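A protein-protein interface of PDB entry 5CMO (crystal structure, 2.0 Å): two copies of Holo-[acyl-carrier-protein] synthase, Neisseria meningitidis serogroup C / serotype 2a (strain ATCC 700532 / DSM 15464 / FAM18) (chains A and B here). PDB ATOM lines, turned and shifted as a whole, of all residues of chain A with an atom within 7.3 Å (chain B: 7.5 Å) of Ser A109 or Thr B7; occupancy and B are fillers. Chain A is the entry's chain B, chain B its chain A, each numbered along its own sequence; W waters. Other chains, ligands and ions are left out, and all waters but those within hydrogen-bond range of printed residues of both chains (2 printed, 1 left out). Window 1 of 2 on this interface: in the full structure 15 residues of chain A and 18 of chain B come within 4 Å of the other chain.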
ATOM      1  N   GLY A   6     -15.774  -3.489 -26.339  1.00  0.00           N
ATOM      2  CA  GLY A   6     -14.798  -4.317 -27.020  1.00  0.00           C
ATOM      3  C   GLY A   6     -15.445  -5.327 -27.942  1.00  0.00           C
ATOM      4  O   GLY A   6     -16.543  -5.818 -27.678  1.00  0.00           O
ATOM      5  N   ALA A  55     -13.319 -13.804 -26.739  1.00  0.00           N
ATOM      6  CA  ALA A  55     -13.916 -13.179 -25.565  1.00  0.00           C
ATOM      7  C   ALA A  55     -12.862 -12.457 -24.728  1.00  0.00           C
ATOM      8  O   ALA A  55     -13.105 -11.365 -24.214  1.00  0.00           O
ATOM      9  CB  ALA A  55     -14.637 -14.222 -24.720  1.00  0.00           C
ATOM     10  N   ALA A  58     -11.694  -9.346 -26.586  1.00  0.00           N
ATOM     11  CA  ALA A  58     -12.750  -8.335 -26.534  1.00  0.00           C
ATOM     12  C   ALA A  58     -12.841  -7.717 -25.145  1.00  0.00           C
ATOM     13  O   ALA A  58     -13.061  -6.515 -25.001  1.00  0.00           O
ATOM     14  CB  ALA A  58     -14.082  -8.944 -26.931  1.00  0.00           C
ATOM     15  N   PRO A  86     -23.335 -16.689 -21.180  1.00  0.00           N
ATOM     16  CA  PRO A  86     -21.902 -16.565 -20.891  1.00  0.00           C
ATOM     17  C   PRO A  86     -21.603 -15.440 -19.907  1.00  0.00           C
ATOM     18  O   PRO A  86     -22.240 -14.390 -19.968  1.00  0.00           O
ATOM     19  CB  PRO A  86     -21.293 -16.261 -22.262  1.00  0.00           C
ATOM     20  CG  PRO A  86     -22.387 -15.593 -23.012  1.00  0.00           C
ATOM     21  CD  PRO A  86     -23.659 -16.238 -22.546  1.00  0.00           C
ATOM     22  N   PHE A  88     -18.157 -13.633 -17.333  1.00  0.00           N
ATOM     23  CA  PHE A  88     -16.737 -13.598 -16.991  1.00  0.00           C
ATOM     24  C   PHE A  88     -16.490 -13.967 -15.530  1.00  0.00           C
ATOM     25  O   PHE A  88     -17.231 -13.550 -14.638  1.00  0.00           O
ATOM     26  CB  PHE A  88     -16.142 -12.213 -17.265  1.00  0.00           C
ATOM     27  CG  PHE A  88     -15.911 -11.917 -18.721  1.00  0.00           C
ATOM     28  CD1 PHE A  88     -14.990 -12.648 -19.454  1.00  0.00           C
ATOM     29  CD2 PHE A  88     -16.597 -10.891 -19.351  1.00  0.00           C
ATOM     30  CE1 PHE A  88     -14.770 -12.371 -20.792  1.00  0.00           C
ATOM     31  CE2 PHE A  88     -16.379 -10.609 -20.687  1.00  0.00           C
ATOM     32  CZ  PHE A  88     -15.466 -11.350 -21.409  1.00  0.00           C
ATOM     33  N   SER A 107     -20.241  -7.226 -19.341  1.00  0.00           N
ATOM     34  CA  SER A 107     -21.174  -8.105 -20.039  1.00  0.00           C
ATOM     35  C   SER A 107     -20.515  -8.737 -21.261  1.00  0.00           C
ATOM     36  O   SER A 107     -19.609  -8.157 -21.854  1.00  0.00           O
ATOM     37  CB  SER A 107     -22.429  -7.336 -20.459  1.00  0.00           C
ATOM     38  OG  SER A 107     -23.159  -6.894 -19.329  1.00  0.00           O
ATOM     39  N   LEU A 108     -20.986  -9.924 -21.632  1.00  0.00           N
ATOM     40  CA  LEU A 108     -20.397 -10.679 -22.729  1.00  0.00           C
ATOM     41  C   LEU A 108     -21.459 -11.337 -23.596  1.00  0.00           C
ATOM     42  O   LEU A 108     -22.465 -11.841 -23.096  1.00  0.00           O
ATOM     43  CB  LEU A 108     -19.441 -11.746 -22.182  1.00  0.00           C
ATOM     44  CG  LEU A 108     -18.910 -12.816 -23.143  1.00  0.00           C
ATOM     45  CD1 LEU A 108     -18.018 -12.204 -24.215  1.00  0.00           C
ATOM     46  CD2 LEU A 108     -18.161 -13.901 -22.377  1.00  0.00           C
ATOM     47  N   SER A 109     -21.229 -11.318 -24.902  1.00  0.00           N
ATOM     48  CA  SER A 109     -21.974 -12.167 -25.815  1.00  0.00           C
ATOM     49  C   SER A 109     -21.033 -12.764 -26.843  1.00  0.00           C
ATOM     50  O   SER A 109     -20.095 -12.108 -27.300  1.00  0.00           O
ATOM     51  CB  SER A 109     -23.090 -11.398 -26.515  1.00  0.00           C
ATOM     52  OG  SER A 109     -23.835 -12.270 -27.347  1.00  0.00           O
ATOM     53  N   MET A 110     -21.301 -14.015 -27.199  1.00  0.00           N
ATOM     54  CA  MET A 110     -20.517 -14.726 -28.192  1.00  0.00           C
ATOM     55  C   MET A 110     -21.442 -15.355 -29.221  1.00  0.00           C
ATOM     56  O   MET A 110     -22.570 -15.733 -28.907  1.00  0.00           O
ATOM     57  CB  MET A 110     -19.656 -15.801 -27.531  1.00  0.00           C
ATOM     58  CG  MET A 110     -18.597 -15.255 -26.590  1.00  0.00           C
ATOM     59  SD  MET A 110     -17.614 -16.555 -25.822  1.00  0.00           S
ATOM     60  CE  MET A 110     -18.850 -17.383 -24.823  1.00  0.00           C
ATOM     61  N   SER A 111     -20.958 -15.450 -30.452  1.00  0.00           N
ATOM     62  CA  SER A 111     -21.671 -16.162 -31.499  1.00  0.00           C
ATOM     63  C   SER A 111     -20.685 -16.716 -32.512  1.00  0.00           C
ATOM     64  O   SER A 111     -19.510 -16.344 -32.521  1.00  0.00           O
ATOM     65  CB  SER A 111     -22.679 -15.252 -32.196  1.00  0.00           C
ATOM     66  OG  SER A 111     -23.454 -15.990 -33.124  1.00  0.00           O
ATOM     67  N   ASP A 112     -21.173 -17.609 -33.364  1.00  0.00           N
ATOM     68  CA  ASP A 112     -20.344 -18.216 -34.390  1.00  0.00           C
ATOM     69  C   ASP A 112     -21.179 -18.586 -35.606  1.00  0.00           C
ATOM     70  O   ASP A 112     -22.361 -18.913 -35.492  1.00  0.00           O
ATOM     71  CB  ASP A 112     -19.639 -19.455 -33.843  1.00  0.00           C
ATOM     72  CG  ASP A 112     -20.604 -20.576 -33.518  1.00  0.00           C
ATOM     73  OD1 ASP A 112     -21.241 -20.520 -32.445  1.00  0.00           O
ATOM     74  OD2 ASP A 112     -20.728 -21.511 -34.336  1.00  0.00           O
ATOM     75  N   LEU A 118     -17.233 -14.683 -33.020  1.00  0.00           N
ATOM     76  CA  LEU A 118     -17.387 -13.271 -32.688  1.00  0.00           C
ATOM     77  C   LEU A 118     -17.707 -13.083 -31.208  1.00  0.00           C
ATOM     78  O   LEU A 118     -18.488 -13.842 -30.642  1.00  0.00           O
ATOM     79  CB  LEU A 118     -18.489 -12.662 -33.559  1.00  0.00           C
ATOM     80  CG  LEU A 118     -19.095 -11.304 -33.205  1.00  0.00           C
ATOM     81  CD1 LEU A 118     -18.060 -10.201 -33.062  1.00  0.00           C
ATOM     82  CD2 LEU A 118     -20.098 -10.938 -34.284  1.00  0.00           C
ATOM     83  N   ALA A 119     -17.094 -12.074 -30.589  1.00  0.00           N
ATOM     84  CA  ALA A 119     -17.402 -11.715 -29.207  1.00  0.00           C
ATOM     85  C   ALA A 119     -17.672 -10.219 -29.081  1.00  0.00           C
ATOM     86  O   ALA A 119     -17.002  -9.403 -29.713  1.00  0.00           O
ATOM     87  CB  ALA A 119     -16.263 -12.123 -28.282  1.00  0.00           C
ATOM     88  N   PHE A 120     -18.672  -9.879 -28.273  1.00  0.00           N
ATOM     89  CA  PHE A 120     -18.977  -8.493 -27.925  1.00  0.00           C
ATOM     90  C   PHE A 120     -18.902  -8.335 -26.412  1.00  0.00           C
ATOM     91  O   PHE A 120     -19.456  -9.151 -25.675  1.00  0.00           O
ATOM     92  CB  PHE A 120     -20.371  -8.084 -28.417  1.00  0.00           C
ATOM     93  CG  PHE A 120     -20.410  -7.616 -29.847  1.00  0.00           C
ATOM     94  CD1 PHE A 120     -20.171  -6.288 -30.162  1.00  0.00           C
ATOM     95  CD2 PHE A 120     -20.709  -8.495 -30.873  1.00  0.00           C
ATOM     96  CE1 PHE A 120     -20.218  -5.852 -31.477  1.00  0.00           C
ATOM     97  CE2 PHE A 120     -20.756  -8.061 -32.187  1.00  0.00           C
ATOM     98  CZ  PHE A 120     -20.511  -6.740 -32.488  1.00  0.00           C
ATOM     99  N   VAL A 121     -18.224  -7.287 -25.955  1.00  0.00           N
ATOM    100  CA  VAL A 121     -18.096  -7.018 -24.528  1.00  0.00           C
ATOM    101  C   VAL A 121     -18.388  -5.551 -24.224  1.00  0.00           C
ATOM    102  O   VAL A 121     -17.979  -4.658 -24.969  1.00  0.00           O
ATOM    103  CB  VAL A 121     -16.686  -7.387 -24.017  1.00  0.00           C
ATOM    104  CG1 VAL A 121     -16.516  -7.001 -22.552  1.00  0.00           C
ATOM    105  CG2 VAL A 121     -16.437  -8.870 -24.201  1.00  0.00           C
ATOM    106  N   VAL A 122     -19.111  -5.320 -23.132  1.00  0.00           N
ATOM    107  CA  VAL A 122     -19.353  -3.973 -22.626  1.00  0.00           C
ATOM    108  C   VAL A 122     -19.003  -3.912 -21.143  1.00  0.00           C
ATOM    109  O   VAL A 122     -19.564  -4.651 -20.333  1.00  0.00           O
ATOM    110  CB  VAL A 122     -20.820  -3.539 -22.824  1.00  0.00           C
ATOM    111  CG1 VAL A 122     -21.050  -2.147 -22.242  1.00  0.00           C
ATOM    112  CG2 VAL A 122     -21.191  -3.559 -24.298  1.00  0.00           C
ATOM    113  N   GLY B   4     -28.460  -7.057 -20.418  1.00  0.00           N
ATOM    114  CA  GLY B   4     -27.618  -8.021 -21.093  1.00  0.00           C
ATOM    115  C   GLY B   4     -27.385  -7.612 -22.529  1.00  0.00           C
ATOM    116  O   GLY B   4     -28.071  -6.733 -23.054  1.00  0.00           O
ATOM    117  N   ILE B   5     -26.397  -8.242 -23.157  1.00  0.00           N
ATOM    118  CA  ILE B   5     -26.095  -7.994 -24.559  1.00  0.00           C
ATOM    119  C   ILE B   5     -26.130  -9.299 -25.331  1.00  0.00           C
ATOM    120  O   ILE B   5     -25.947 -10.379 -24.763  1.00  0.00           O
ATOM    121  CB  ILE B   5     -24.717  -7.321 -24.740  1.00  0.00           C
ATOM    122  CG1 ILE B   5     -23.598  -8.202 -24.171  1.00  0.00           C
ATOM    123  CG2 ILE B   5     -24.713  -5.963 -24.066  1.00  0.00           C
ATOM    124  CD1 ILE B   5     -22.203  -7.671 -24.435  1.00  0.00           C
ATOM    125  N   GLY B   6     -26.366  -9.186 -26.631  1.00  0.00           N
ATOM    126  CA  GLY B   6     -26.456 -10.343 -27.493  1.00  0.00           C
ATOM    127  C   GLY B   6     -25.959 -10.042 -28.889  1.00  0.00           C
ATOM    128  O   GLY B   6     -26.057  -8.911 -29.365  1.00  0.00           O
ATOM    129  N   THR B   7     -25.411 -11.059 -29.542  1.00  0.00           N
ATOM    130  CA  THR B   7     -25.012 -10.936 -30.934  1.00  0.00           C
ATOM    131  C   THR B   7     -25.219 -12.252 -31.660  1.00  0.00           C
ATOM    132  O   THR B   7     -25.237 -13.319 -31.045  1.00  0.00           O
ATOM    133  CB  THR B   7     -23.537 -10.510 -31.079  1.00  0.00           C
ATOM    134  OG1 THR B   7     -23.238 -10.283 -32.462  1.00  0.00           O
ATOM    135  CG2 THR B   7     -22.604 -11.586 -30.531  1.00  0.00           C
ATOM    136  N   ASP B   8     -25.379 -12.167 -32.974  1.00  0.00           N
ATOM    137  CA  ASP B   8     -25.424 -13.355 -33.809  1.00  0.00           C
ATOM    138  C   ASP B   8     -25.051 -12.990 -35.233  1.00  0.00           C
ATOM    139  O   ASP B   8     -25.352 -11.890 -35.704  1.00  0.00           O
ATOM    140  CB  ASP B   8     -26.809 -14.004 -33.772  1.00  0.00           C
ATOM    141  CG  ASP B   8     -26.817 -15.392 -34.384  1.00  0.00           C
ATOM    142  OD1 ASP B   8     -25.853 -16.152 -34.156  1.00  0.00           O
ATOM    143  OD2 ASP B   8     -27.785 -15.724 -35.098  1.00  0.00           O
ATOM    144  N   ILE B   9     -24.375 -13.914 -35.906  1.00  0.00           N
ATOM    145  CA  ILE B   9     -24.014 -13.739 -37.306  1.00  0.00           C
ATOM    146  C   ILE B   9     -24.613 -14.883 -38.114  1.00  0.00           C
ATOM    147  O   ILE B   9     -24.636 -16.031 -37.661  1.00  0.00           O
ATOM    148  CB  ILE B   9     -22.484 -13.677 -37.501  1.00  0.00           C
ATOM    149  CG1 ILE B   9     -21.796 -14.777 -36.688  1.00  0.00           C
ATOM    150  CG2 ILE B   9     -21.961 -12.309 -37.079  1.00  0.00           C
ATOM    151  CD1 ILE B   9     -20.299 -14.842 -36.884  1.00  0.00           C
ATOM    152  N   ALA B  54     -30.923 -13.823 -37.287  1.00  0.00           N
ATOM    153  CA  ALA B  54     -29.826 -13.242 -36.511  1.00  0.00           C
ATOM    154  C   ALA B  54     -30.329 -12.366 -35.366  1.00  0.00           C
ATOM    155  O   ALA B  54     -29.856 -12.473 -34.235  1.00  0.00           O
ATOM    156  CB  ALA B  54     -28.912 -12.427 -37.419  1.00  0.00           C
ATOM    157  N   ALA B  55     -31.280 -11.491 -35.673  1.00  0.00           N
ATOM    158  CA  ALA B  55     -31.815 -10.551 -34.693  1.00  0.00           C
ATOM    159  C   ALA B  55     -32.491 -11.261 -33.523  1.00  0.00           C
ATOM    160  O   ALA B  55     -32.301 -10.887 -32.364  1.00  0.00           O
ATOM    161  CB  ALA B  55     -32.797  -9.608 -35.365  1.00  0.00           C
ATOM    162  N   GLU B  57     -32.044 -14.417 -32.493  1.00  0.00           N
ATOM    163  CA  GLU B  57     -31.040 -15.136 -31.719  1.00  0.00           C
ATOM    164  C   GLU B  57     -30.279 -14.173 -30.807  1.00  0.00           C
ATOM    165  O   GLU B  57     -30.017 -14.479 -29.644  1.00  0.00           O
ATOM    166  CB  GLU B  57     -30.070 -15.873 -32.647  1.00  0.00           C
ATOM    167  CG  GLU B  57     -30.614 -17.187 -33.195  1.00  0.00           C
ATOM    168  CD  GLU B  57     -30.744 -18.263 -32.131  1.00  0.00           C
ATOM    169  OE1 GLU B  57     -30.025 -18.194 -31.111  1.00  0.00           O
ATOM    170  OE2 GLU B  57     -31.569 -19.183 -32.314  1.00  0.00           O
ATOM    171  N   ALA B  58     -29.940 -13.002 -31.337  1.00  0.00           N
ATOM    172  CA  ALA B  58     -29.221 -11.995 -30.563  1.00  0.00           C
ATOM    173  C   ALA B  58     -30.099 -11.445 -29.444  1.00  0.00           C
ATOM    174  O   ALA B  58     -29.613 -11.130 -28.359  1.00  0.00           O
ATOM    175  CB  ALA B  58     -28.749 -10.869 -31.468  1.00  0.00           C
ATOM    176  N   PHE B  59     -31.393 -11.325 -29.715  1.00  0.00           N
ATOM    177  CA  PHE B  59     -32.337 -10.872 -28.703  1.00  0.00           C
ATOM    178  C   PHE B  59     -32.385 -11.867 -27.549  1.00  0.00           C
ATOM    179  O   PHE B  59     -32.304 -11.487 -26.380  1.00  0.00           O
ATOM    180  CB  PHE B  59     -33.734 -10.696 -29.302  1.00  0.00           C
ATOM    181  CG  PHE B  59     -34.781 -10.314 -28.292  1.00  0.00           C
ATOM    182  CD1 PHE B  59     -35.457 -11.284 -27.570  1.00  0.00           C
ATOM    183  CD2 PHE B  59     -35.090  -8.983 -28.068  1.00  0.00           C
ATOM    184  CE1 PHE B  59     -36.418 -10.933 -26.640  1.00  0.00           C
ATOM    185  CE2 PHE B  59     -36.050  -8.626 -27.141  1.00  0.00           C
ATOM    186  CZ  PHE B  59     -36.716  -9.604 -26.427  1.00  0.00           C
ATOM    187  N   LYS B  61     -30.255 -14.000 -26.545  1.00  0.00           N
ATOM    188  CA  LYS B  61     -29.027 -13.980 -25.759  1.00  0.00           C
ATOM    189  C   LYS B  61     -28.986 -12.755 -24.848  1.00  0.00           C
ATOM    190  O   LYS B  61     -28.567 -12.840 -23.693  1.00  0.00           O
ATOM    191  CB  LYS B  61     -27.803 -13.989 -26.678  1.00  0.00           C
ATOM    192  CG  LYS B  61     -27.597 -15.289 -27.437  1.00  0.00           C
ATOM    193  CD  LYS B  61     -26.376 -15.200 -28.331  1.00  0.00           C
ATOM    194  CE  LYS B  61     -26.253 -16.413 -29.230  1.00  0.00           C
ATOM    195  NZ  LYS B  61     -25.100 -16.283 -30.160  1.00  0.00           N
ATOM    196  N   ALA B  62     -29.431 -11.620 -25.376  1.00  0.00           N
ATOM    197  CA  ALA B  62     -29.378 -10.356 -24.648  1.00  0.00           C
ATOM    198  C   ALA B  62     -30.263 -10.361 -23.404  1.00  0.00           C
ATOM    199  O   ALA B  62     -29.943  -9.707 -22.411  1.00  0.00           O
ATOM    200  CB  ALA B  62     -29.776  -9.212 -25.563  1.00  0.00           C
ATOM    201  N   SER B 109     -29.092  -3.292 -33.540  1.00  0.00           N
ATOM    202  CA  SER B 109     -28.199  -2.812 -34.590  1.00  0.00           C
ATOM    203  C   SER B 109     -27.911  -3.945 -35.559  1.00  0.00           C
ATOM    204  O   SER B 109     -27.555  -5.049 -35.142  1.00  0.00           O
ATOM    205  CB  SER B 109     -26.891  -2.278 -34.004  1.00  0.00           C
ATOM    206  OG  SER B 109     -26.016  -1.841 -35.031  1.00  0.00           O
ATOM    207  N   LEU B 118     -25.134  -9.533 -39.642  1.00  0.00           N
ATOM    208  CA  LEU B 118     -24.796  -9.414 -38.229  1.00  0.00           C
ATOM    209  C   LEU B 118     -25.849  -8.620 -37.465  1.00  0.00           C
ATOM    210  O   LEU B 118     -26.329  -7.589 -37.936  1.00  0.00           O
ATOM    211  CB  LEU B 118     -23.423  -8.754 -38.071  1.00  0.00           C
ATOM    212  CG  LEU B 118     -22.970  -8.451 -36.639  1.00  0.00           C
ATOM    213  CD1 LEU B 118     -21.480  -8.691 -36.494  1.00  0.00           C
ATOM    214  CD2 LEU B 118     -23.305  -7.019 -36.247  1.00  0.00           C
ATOM    215  N   ALA B 119     -26.197  -9.120 -36.282  1.00  0.00           N
ATOM    216  CA  ALA B 119     -27.113  -8.434 -35.379  1.00  0.00           C
ATOM    217  C   ALA B 119     -26.453  -8.254 -34.024  1.00  0.00           C
ATOM    218  O   ALA B 119     -25.838  -9.185 -33.502  1.00  0.00           O
ATOM    219  CB  ALA B 119     -28.409  -9.211 -35.234  1.00  0.00           C
ATOM    220  N   PHE B 120     -26.563  -7.053 -33.469  1.00  0.00           N
ATOM    221  CA  PHE B 120     -26.144  -6.801 -32.097  1.00  0.00           C
ATOM    222  C   PHE B 120     -27.294  -6.180 -31.322  1.00  0.00           C
ATOM    223  O   PHE B 120     -27.960  -5.264 -31.808  1.00  0.00           O
ATOM    224  CB  PHE B 120     -24.919  -5.891 -32.042  1.00  0.00           C
ATOM    225  CG  PHE B 120     -24.457  -5.595 -30.643  1.00  0.00           C
ATOM    226  CD1 PHE B 120     -23.925  -6.600 -29.850  1.00  0.00           C
ATOM    227  CD2 PHE B 120     -24.557  -4.319 -30.119  1.00  0.00           C
ATOM    228  CE1 PHE B 120     -23.502  -6.335 -28.561  1.00  0.00           C
ATOM    229  CE2 PHE B 120     -24.135  -4.049 -28.832  1.00  0.00           C
ATOM    230  CZ  PHE B 120     -23.606  -5.058 -28.052  1.00  0.00           C
ATOM    231  N   VAL B 121     -27.514  -6.690 -30.116  1.00  0.00           N
ATOM    232  CA  VAL B 121     -28.649  -6.285 -29.302  1.00  0.00           C
ATOM    233  C   VAL B 121     -28.219  -5.949 -27.874  1.00  0.00           C
ATOM    234  O   VAL B 121     -27.435  -6.674 -27.258  1.00  0.00           O
ATOM    235  CB  VAL B 121     -29.725  -7.392 -29.273  1.00  0.00           C
ATOM    236  CG1 VAL B 121     -30.836  -7.043 -28.296  1.00  0.00           C
ATOM    237  CG2 VAL B 121     -30.297  -7.616 -30.670  1.00  0.00           C
ATOM    238  N   VAL B 122     -28.749  -4.842 -27.362  1.00  0.00           N
ATOM    239  CA  VAL B 122     -28.555  -4.452 -25.971  1.00  0.00           C
ATOM    240  C   VAL B 122     -29.900  -4.299 -25.273  1.00  0.00           C
ATOM    241  O   VAL B 122     -30.701  -3.438 -25.635  1.00  0.00           O
ATOM    242  CB  VAL B 122     -27.783  -3.127 -25.848  1.00  0.00           C
ATOM    243  CG1 VAL B 122     -27.635  -2.727 -24.380  1.00  0.00           C
ATOM    244  CG2 VAL B 122     -26.423  -3.243 -26.499  1.00  0.00           C
HETATM  245  O   HOH W   1     -24.879 -12.882 -23.705  1.00  0.00           O
HETATM  246  O   HOH W   2     -25.004 -10.249 -21.293  1.00  0.00           O
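The backbone NH (N) of Val B121 lies within hydrogen-bond range of the backbone carbonyl oxygen (O) of Gly B6.
NZ of Lys B61 lies within hydrogen-bond range of O of Thr B7.
The backbone carbonyl oxygen of Asp B8 is in hydrogen-bond range of the backbone NH of Ala B119 (3.0 Å).
The backbone NH (N) of Phe B120 lies within hydrogen-bond range of the backbone carbonyl oxygen (O) of Ser B109 (2.8 Å).
N of Ser A107 sits at hydrogen-bond distance from O of Val A122, 2.8 Å away.
The backbone carbonyl oxygen (O) of Ser A111 lies within hydrogen-bond range of the backbone NH (N) of Leu A118 (2.9 Å).
Water W1 bridges the backbone carbonyl oxygen of Leu A108 and the backbone carbonyl oxygen of Ile B5.
Water W2 lies within hydrogen-bond range of N of Ile B5 (3.1 Å) and O of Leu A108 (3.5 Å).
The backbone NH of Thr B7 sits at hydrogen-bond distance from the side-chain hydroxyl of Ser A109 (3.0 Å).
OD1 of Asp B8 is in hydrogen-bond range of OG of Ser A111 (2.6 Å).
The side-chain amino group (NZ) of Lys B61 lies within hydrogen-bond range of the backbone carbonyl oxygen (O) of Met A110 (2.9 Å).
The side-chain hydroxyl (OG) of Ser A111 lies close to the side-chain amino group (NZ) of Lys B61, 3.4 Å away.
Ser A109 touches Gly B6, but with the chains exchanged Gly A6 does not touch Ser B109 (12.6 Å).
Leu B118 touches its own counterpart, Leu A118.
Phe A120 touches its own counterpart, Phe B120.
Positions printed for both chains: 6, 55, 58, 109, 118, 119, 120, 121 and 122.
Of the 16 pairs that touch across the chains among the printed residues, 2 have their exchanged pair printed and touching as well.
Among the printed residues, pairs that only touch across the chains: Ser A109 with Gly B6, Phe A120 with Thr B7, Phe A120 with Ile B5, Ser A111 with Thr B7, Leu A118 with Leu B118, Ser A109 with Ile B5, Phe A120 with Phe B120, Ser A111 with Ile B9, Leu A118 with Ile B9, Leu A118 with Thr B7, Ser A107 with Ile B5 and Leu A108 with Ile B5.
Of the 19 printed residues of chain B, 8 touch a printed residue of chain A.
Hydrophobic or aromatic side chains of chain B that line the printed part of chain A: Ile B5, Ile B9, Leu B118 and Phe B120.
Along chain B the printed residues that touch a printed residue of chain A span positions 5 to 120.
Among the printed residues, 16 pairs touch across the chains.
Among the printed residues, no Asp or Glu carboxylate lies within 4 Å of a Lys or Arg side-chain nitrogen of the other chain.
Printed residues of chain B within 4 Å of Leu A108: Ile B5.
Printed residues of chain B within 4 Å of Ser A109: Ile B5 (3.5 Å), Gly B6 (3.3 Å) and Thr B7 (3.0 Å).
Printed residues of chain B within 4 Å of Leu A118: Thr B7 (3.7 Å), Ile B9 (3.6 Å) and Leu B118 (3.4 Å).
Printed residues of chain A within 4 Å of Ile B5: Ser A107, Leu A108, Ser A109 and Phe A120.
Thr B7 touches just these residues of chain A: Ser A109, Ser A111, Leu A118 and Phe A120.
Printed residues of chain A within 4 Å of Asp B8: Ser A111.
Ser B109 touches none of the printed residues of chain A.
Val B122 touches none of the printed residues of chain A.
The nearest printed residue of chain A that does not touch Gly B6 is Phe A120 (5.6 Å).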
